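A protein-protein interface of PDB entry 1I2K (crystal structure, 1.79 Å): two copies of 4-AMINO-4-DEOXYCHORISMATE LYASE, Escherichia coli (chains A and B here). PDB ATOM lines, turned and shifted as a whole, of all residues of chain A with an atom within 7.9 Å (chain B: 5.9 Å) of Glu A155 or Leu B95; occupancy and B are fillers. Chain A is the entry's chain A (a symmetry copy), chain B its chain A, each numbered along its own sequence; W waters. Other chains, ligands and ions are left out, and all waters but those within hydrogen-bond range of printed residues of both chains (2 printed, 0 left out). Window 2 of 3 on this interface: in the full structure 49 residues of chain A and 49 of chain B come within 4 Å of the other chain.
The guanidinium group of Arg A151 is in salt-bridge range of the side-chain carboxylate of Glu A155. The side-chain hydroxyl (OG) of Ser B97 sits at hydrogen-bond distance from the backbone carbonyl oxygen (O) of Thr B94 (2.8 Å). OG of Ser B93 is in hydrogen-bond range of N of Leu B95.
No position is printed for both chains.
Of the 8 printed residues of chain B, 3 touch a printed residue of chain A. Printed residues of chain B that touch a printed residue of chain A: Ser B93, Thr B94 and Leu B95. Hydrophobic or aromatic side chains of chain B that line the printed part of chain A: Leu B95. Printed residues of chain A that touch a printed residue of chain B: Val A148, Arg A151 and Glu A155. Among the printed residues, no Asp or Glu carboxylate lies within 4 Å of a Lys or Arg side-chain nitrogen of the other chain.
Val A148 touches Thr B94 (CG1 to CG2, 3.7 Å). Ser B93 touches Arg A151 (CA to CG, 3.6 Å). Leu B95 touches Glu A155 (CG to OE1, 3.5 Å).
The side-chain carboxylate (OE2) of Glu A155 is in hydrogen-bond range of the side-chain hydroxyl (OG) of Ser B93 (2.5 Å).
Glu A155 touches just these residues of chain B: Ser B93 and Leu B95. Of chain A, only Glu A155 (3.5 Å) comes within 4 Å of Leu B95. Printed residues of chain A within 4 Å of Ser B93: Arg A151 (3.6 Å) and Glu A155 (2.5 Å). Printed residues of chain B within 4 Å of Arg A151: Ser B93. Of the printed residues of chain B, Val A148 touches Thr B94 (3.7 Å). Ile A150 touches none of the printed residues of chain B. Leu A149 touches none of the printed residues of chain B. The nearest printed residue of chain A that does not touch Leu B95 is Arg A151 (6.9 Å).
Water W2 lies within hydrogen-bond range of the side-chain carboxylate (OE1) of Glu A155 (2.5 Å) and the backbone NH (N) of Thr B94 (2.7 Å). Water W1 lies within hydrogen-bond range of O of Arg B90 (2.8 Å) and NE of Arg A151 (3.5 Å).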
ATOM      1  N   ALA A 124      14.407 -10.711 -22.565  1.00  0.00           N
ATOM      2  CA  ALA A 124      15.012 -11.280 -23.755  1.00  0.00           C
ATOM      3  C   ALA A 124      14.926 -10.306 -24.934  1.00  0.00           C
ATOM      4  O   ALA A 124      13.875  -9.716 -25.179  1.00  0.00           O
ATOM      5  CB  ALA A 124      14.343 -12.584 -24.157  1.00  0.00           C
ATOM      6  N   VAL A 148       1.835  -7.518 -30.600  1.00  0.00           N
ATOM      7  CA  VAL A 148       1.409  -8.934 -30.642  1.00  0.00           C
ATOM      8  C   VAL A 148       2.532  -9.837 -31.134  1.00  0.00           C
ATOM      9  O   VAL A 148       2.797 -10.936 -30.623  1.00  0.00           O
ATOM     10  CB  VAL A 148       0.180  -9.107 -31.553  1.00  0.00           C
ATOM     11  CG1 VAL A 148      -0.123 -10.585 -31.782  1.00  0.00           C
ATOM     12  CG2 VAL A 148      -1.014  -8.392 -30.934  1.00  0.00           C
ATOM     13  N   LEU A 149       3.230  -9.405 -32.187  1.00  0.00           N
ATOM     14  CA  LEU A 149       4.365 -10.204 -32.669  1.00  0.00           C
ATOM     15  C   LEU A 149       5.522 -10.297 -31.679  1.00  0.00           C
ATOM     16  O   LEU A 149       6.123 -11.370 -31.535  1.00  0.00           O
ATOM     17  CB  LEU A 149       4.899  -9.617 -33.979  1.00  0.00           C
ATOM     18  CG  LEU A 149       3.935  -9.729 -35.176  1.00  0.00           C
ATOM     19  CD1 LEU A 149       4.560  -9.151 -36.446  1.00  0.00           C
ATOM     20  CD2 LEU A 149       3.514 -11.171 -35.386  1.00  0.00           C
ATOM     21  N   ILE A 150       5.865  -9.212 -30.997  1.00  0.00           N
ATOM     22  CA  ILE A 150       6.884  -9.213 -29.941  1.00  0.00           C
ATOM     23  C   ILE A 150       6.522 -10.189 -28.840  1.00  0.00           C
ATOM     24  O   ILE A 150       7.330 -10.985 -28.349  1.00  0.00           O
ATOM     25  CB  ILE A 150       7.058  -7.775 -29.397  1.00  0.00           C
ATOM     26  CG1 ILE A 150       7.731  -6.836 -30.405  1.00  0.00           C
ATOM     27  CG2 ILE A 150       7.786  -7.746 -28.062  1.00  0.00           C
ATOM     28  CD1 ILE A 150       7.633  -5.359 -30.116  1.00  0.00           C
ATOM     29  N   ARG A 151       5.271 -10.152 -28.379  1.00  0.00           N
ATOM     30  CA  ARG A 151       4.853 -11.050 -27.310  1.00  0.00           C
ATOM     31  C   ARG A 151       5.041 -12.497 -27.761  1.00  0.00           C
ATOM     32  O   ARG A 151       5.493 -13.339 -26.983  1.00  0.00           O
ATOM     33  CB  ARG A 151       3.388 -10.824 -26.930  1.00  0.00           C
ATOM     34  CG  ARG A 151       2.922 -11.608 -25.715  1.00  0.00           C
ATOM     35  CD  ARG A 151       3.696 -11.242 -24.457  1.00  0.00           C
ATOM     36  NE  ARG A 151       3.515 -12.263 -23.424  1.00  0.00           N
ATOM     37  CZ  ARG A 151       3.896 -12.099 -22.160  1.00  0.00           C
ATOM     38  NH1 ARG A 151       4.475 -10.958 -21.797  1.00  0.00           N
ATOM     39  NH2 ARG A 151       3.702 -13.066 -21.271  1.00  0.00           N
ATOM     40  N   SER A 152       4.686 -12.749 -29.022  1.00  0.00           N
ATOM     41  CA  SER A 152       4.703 -14.105 -29.545  1.00  0.00           C
ATOM     42  C   SER A 152       6.129 -14.649 -29.595  1.00  0.00           C
ATOM     43  O   SER A 152       6.389 -15.812 -29.246  1.00  0.00           O
ATOM     44  CB  SER A 152       4.086 -14.245 -30.942  1.00  0.00           C
ATOM     45  OG  SER A 152       3.956 -15.642 -31.198  1.00  0.00           O
ATOM     46  N   HIS A 153       7.049 -13.794 -30.018  1.00  0.00           N
ATOM     47  CA  HIS A 153       8.434 -14.271 -30.006  1.00  0.00           C
ATOM     48  C   HIS A 153       8.973 -14.438 -28.591  1.00  0.00           C
ATOM     49  O   HIS A 153       9.800 -15.327 -28.305  1.00  0.00           O
ATOM     50  CB  HIS A 153       9.308 -13.323 -30.826  1.00  0.00           C
ATOM     51  CG  HIS A 153       9.033 -13.307 -32.297  1.00  0.00           C
ATOM     52  ND1 HIS A 153       9.898 -13.854 -33.220  1.00  0.00           N
ATOM     53  CD2 HIS A 153       8.003 -12.811 -33.019  1.00  0.00           C
ATOM     54  CE1 HIS A 153       9.410 -13.690 -34.447  1.00  0.00           C
ATOM     55  NE2 HIS A 153       8.262 -13.067 -34.349  1.00  0.00           N
ATOM     56  N   LEU A 154       8.548 -13.596 -27.667  1.00  0.00           N
ATOM     57  CA  LEU A 154       8.964 -13.642 -26.268  1.00  0.00           C
ATOM     58  C   LEU A 154       8.557 -14.950 -25.605  1.00  0.00           C
ATOM     59  O   LEU A 154       9.209 -15.534 -24.736  1.00  0.00           O
ATOM     60  CB  LEU A 154       8.386 -12.467 -25.469  1.00  0.00           C
ATOM     61  CG  LEU A 154       8.761 -12.499 -23.979  1.00  0.00           C
ATOM     62  CD1 LEU A 154      10.233 -12.149 -23.814  1.00  0.00           C
ATOM     63  CD2 LEU A 154       7.865 -11.567 -23.183  1.00  0.00           C
ATOM     64  N   GLU A 155       7.382 -15.425 -25.993  1.00  0.00           N
ATOM     65  CA  GLU A 155       6.888 -16.638 -25.332  1.00  0.00           C
ATOM     66  C   GLU A 155       7.729 -17.849 -25.692  1.00  0.00           C
ATOM     67  O   GLU A 155       7.637 -18.912 -25.072  1.00  0.00           O
ATOM     68  CB  GLU A 155       5.396 -16.756 -25.695  1.00  0.00           C
ATOM     69  CG  GLU A 155       4.586 -15.708 -24.913  1.00  0.00           C
ATOM     70  CD  GLU A 155       3.147 -15.614 -25.378  1.00  0.00           C
ATOM     71  OE1 GLU A 155       2.856 -16.137 -26.473  1.00  0.00           O
ATOM     72  OE2 GLU A 155       2.292 -15.032 -24.682  1.00  0.00           O
ATOM     73  N   GLN A 156       8.610 -17.759 -26.698  1.00  0.00           N
ATOM     74  CA  GLN A 156       9.423 -18.918 -27.047  1.00  0.00           C
ATOM     75  C   GLN A 156      10.702 -18.975 -26.203  1.00  0.00           C
ATOM     76  O   GLN A 156      11.567 -19.804 -26.482  1.00  0.00           O
ATOM     77  CB  GLN A 156       9.826 -18.939 -28.521  1.00  0.00           C
ATOM     78  CG  GLN A 156       8.728 -18.678 -29.516  1.00  0.00           C
ATOM     79  CD  GLN A 156       7.953 -19.879 -29.995  1.00  0.00           C
ATOM     80  OE1 GLN A 156       8.497 -20.964 -30.176  1.00  0.00           O
ATOM     81  NE2 GLN A 156       6.652 -19.674 -30.205  1.00  0.00           N
ATOM     82  N   THR A 157      10.786 -18.107 -25.212  1.00  0.00           N
ATOM     83  CA  THR A 157      11.879 -18.034 -24.255  1.00  0.00           C
ATOM     84  C   THR A 157      11.394 -18.273 -22.825  1.00  0.00           C
ATOM     85  O   THR A 157      10.212 -18.564 -22.620  1.00  0.00           O
ATOM     86  CB  THR A 157      12.576 -16.662 -24.313  1.00  0.00           C
ATOM     87  OG1 THR A 157      11.684 -15.692 -23.737  1.00  0.00           O
ATOM     88  CG2 THR A 157      12.886 -16.243 -25.749  1.00  0.00           C
ATOM     89  N   ASN A 158      12.293 -18.138 -21.858  1.00  0.00           N
ATOM     90  CA  ASN A 158      12.028 -18.206 -20.427  1.00  0.00           C
ATOM     91  C   ASN A 158      12.033 -16.808 -19.797  1.00  0.00           C
ATOM     92  O   ASN A 158      12.120 -16.681 -18.574  1.00  0.00           O
ATOM     93  CB  ASN A 158      13.055 -19.084 -19.711  1.00  0.00           C
ATOM     94  CG  ASN A 158      12.611 -19.577 -18.349  1.00  0.00           C
ATOM     95  OD1 ASN A 158      13.444 -19.924 -17.501  1.00  0.00           O
ATOM     96  ND2 ASN A 158      11.301 -19.618 -18.119  1.00  0.00           N
ATOM     97  N   ALA A 159      11.952 -15.792 -20.645  1.00  0.00           N
ATOM     98  CA  ALA A 159      11.913 -14.387 -20.279  1.00  0.00           C
ATOM     99  C   ALA A 159      10.490 -13.932 -19.984  1.00  0.00           C
ATOM    100  O   ALA A 159       9.538 -14.464 -20.563  1.00  0.00           O
ATOM    101  CB  ALA A 159      12.522 -13.536 -21.382  1.00  0.00           C
ATOM    102  N   ASP A 160      10.345 -12.949 -19.089  1.00  0.00           N
ATOM    103  CA  ASP A 160       9.019 -12.467 -18.721  1.00  0.00           C
ATOM    104  C   ASP A 160       8.636 -11.227 -19.518  1.00  0.00           C
ATOM    105  O   ASP A 160       7.468 -10.899 -19.673  1.00  0.00           O
ATOM    106  CB  ASP A 160       8.975 -12.099 -17.244  1.00  0.00           C
ATOM    107  CG  ASP A 160       9.498 -13.235 -16.376  1.00  0.00           C
ATOM    108  OD1 ASP A 160       8.764 -14.236 -16.280  1.00  0.00           O
ATOM    109  OD2 ASP A 160      10.604 -13.141 -15.820  1.00  0.00           O
ATOM    110  N   ALA A 162      10.338  -8.422 -22.859  1.00  0.00           N
ATOM    111  CA  ALA A 162      11.274  -8.252 -23.952  1.00  0.00           C
ATOM    112  C   ALA A 162      12.036  -6.934 -23.889  1.00  0.00           C
ATOM    113  O   ALA A 162      11.497  -5.952 -23.382  1.00  0.00           O
ATOM    114  CB  ALA A 162      10.496  -8.270 -25.270  1.00  0.00           C
ATOM    115  N   GLY B  88      -9.840 -13.167 -26.982  1.00  0.00           N
ATOM    116  CA  GLY B  88      -9.112 -13.961 -26.005  1.00  0.00           C
ATOM    117  C   GLY B  88      -7.688 -13.523 -25.763  1.00  0.00           C
ATOM    118  O   GLY B  88      -7.239 -12.530 -26.341  1.00  0.00           O
ATOM    119  N   GLY B  89      -6.998 -14.280 -24.910  1.00  0.00           N
ATOM    120  CA  GLY B  89      -5.570 -14.100 -24.705  1.00  0.00           C
ATOM    121  C   GLY B  89      -5.350 -13.051 -23.631  1.00  0.00           C
ATOM    122  O   GLY B  89      -6.229 -12.196 -23.466  1.00  0.00           O
ATOM    123  N   ARG B  90      -4.238 -13.138 -22.920  1.00  0.00           N
ATOM    124  CA  ARG B  90      -4.000 -12.145 -21.864  1.00  0.00           C
ATOM    125  C   ARG B  90      -3.108 -11.020 -22.378  1.00  0.00           C
ATOM    126  O   ARG B  90      -1.998 -11.253 -22.864  1.00  0.00           O
ATOM    127  CB  ARG B  90      -3.379 -12.769 -20.612  1.00  0.00           C
ATOM    128  CG  ARG B  90      -2.265 -13.763 -20.878  1.00  0.00           C
ATOM    129  CD  ARG B  90      -1.160 -13.673 -19.838  1.00  0.00           C
ATOM    130  NE  ARG B  90      -1.441 -14.459 -18.642  1.00  0.00           N
ATOM    131  CZ  ARG B  90      -0.498 -14.910 -17.820  1.00  0.00           C
ATOM    132  NH1 ARG B  90       0.776 -14.649 -18.080  1.00  0.00           N
ATOM    133  NH2 ARG B  90      -0.855 -15.614 -16.757  1.00  0.00           N
ATOM    134  N   SER B  93      -0.861 -11.298 -25.589  1.00  0.00           N
ATOM    135  CA  SER B  93      -0.474 -12.675 -25.919  1.00  0.00           C
ATOM    136  C   SER B  93      -1.526 -13.353 -26.791  1.00  0.00           C
ATOM    137  O   SER B  93      -2.716 -13.100 -26.529  1.00  0.00           O
ATOM    138  CB  SER B  93      -0.250 -13.494 -24.634  1.00  0.00           C
ATOM    139  OG  SER B  93      -0.174 -14.888 -24.922  1.00  0.00           O
ATOM    140  N   THR B  94      -1.102 -14.182 -27.757  1.00  0.00           N
ATOM    141  CA  THR B  94      -2.046 -14.969 -28.554  1.00  0.00           C
ATOM    142  C   THR B  94      -2.350 -16.334 -27.956  1.00  0.00           C
ATOM    143  O   THR B  94      -3.107 -17.147 -28.496  1.00  0.00           O
ATOM    144  CB  THR B  94      -1.520 -15.245 -29.969  1.00  0.00           C
ATOM    145  OG1 THR B  94      -0.404 -16.145 -29.895  1.00  0.00           O
ATOM    146  CG2 THR B  94      -0.983 -13.953 -30.582  1.00  0.00           C
ATOM    147  N   LEU B  95      -1.754 -16.630 -26.809  1.00  0.00           N
ATOM    148  CA  LEU B  95      -2.019 -17.929 -26.194  1.00  0.00           C
ATOM    149  C   LEU B  95      -3.445 -18.039 -25.661  1.00  0.00           C
ATOM    150  O   LEU B  95      -3.859 -17.126 -24.943  1.00  0.00           O
ATOM    151  CB  LEU B  95      -1.015 -18.139 -25.053  1.00  0.00           C
ATOM    152  CG  LEU B  95       0.395 -18.458 -25.556  1.00  0.00           C
ATOM    153  CD1 LEU B  95       1.297 -18.750 -24.365  1.00  0.00           C
ATOM    154  CD2 LEU B  95       0.369 -19.628 -26.517  1.00  0.00           C
ATOM    155  N   ASN B  96      -4.130 -19.117 -26.007  1.00  0.00           N
ATOM    156  CA  ASN B  96      -5.500 -19.454 -25.656  1.00  0.00           C
ATOM    157  C   ASN B  96      -6.513 -18.552 -26.349  1.00  0.00           C
ATOM    158  O   ASN B  96      -7.687 -18.511 -25.987  1.00  0.00           O
ATOM    159  CB  ASN B  96      -5.730 -19.402 -24.132  1.00  0.00           C
ATOM    160  CG  ASN B  96      -4.725 -20.282 -23.403  1.00  0.00           C
ATOM    161  OD1 ASN B  96      -4.518 -21.440 -23.770  1.00  0.00           O
ATOM    162  ND2 ASN B  96      -4.074 -19.723 -22.386  1.00  0.00           N
ATOM    163  N   SER B  97      -6.114 -17.808 -27.371  1.00  0.00           N
ATOM    164  CA  SER B  97      -7.082 -16.957 -28.074  1.00  0.00           C
ATOM    165  C   SER B  97      -7.759 -17.691 -29.215  1.00  0.00           C
ATOM    166  O   SER B  97      -7.282 -18.719 -29.689  1.00  0.00           O
ATOM    167  CB  SER B  97      -6.359 -15.722 -28.637  1.00  0.00           C
ATOM    168  OG  SER B  97      -5.456 -16.181 -29.643  1.00  0.00           O
HETATM  169  O   HOH W   1       0.571 -11.375 -21.771  1.00  0.00           O
HETATM  170  O   HOH W   2       1.487 -14.857 -28.083  1.00  0.00           O
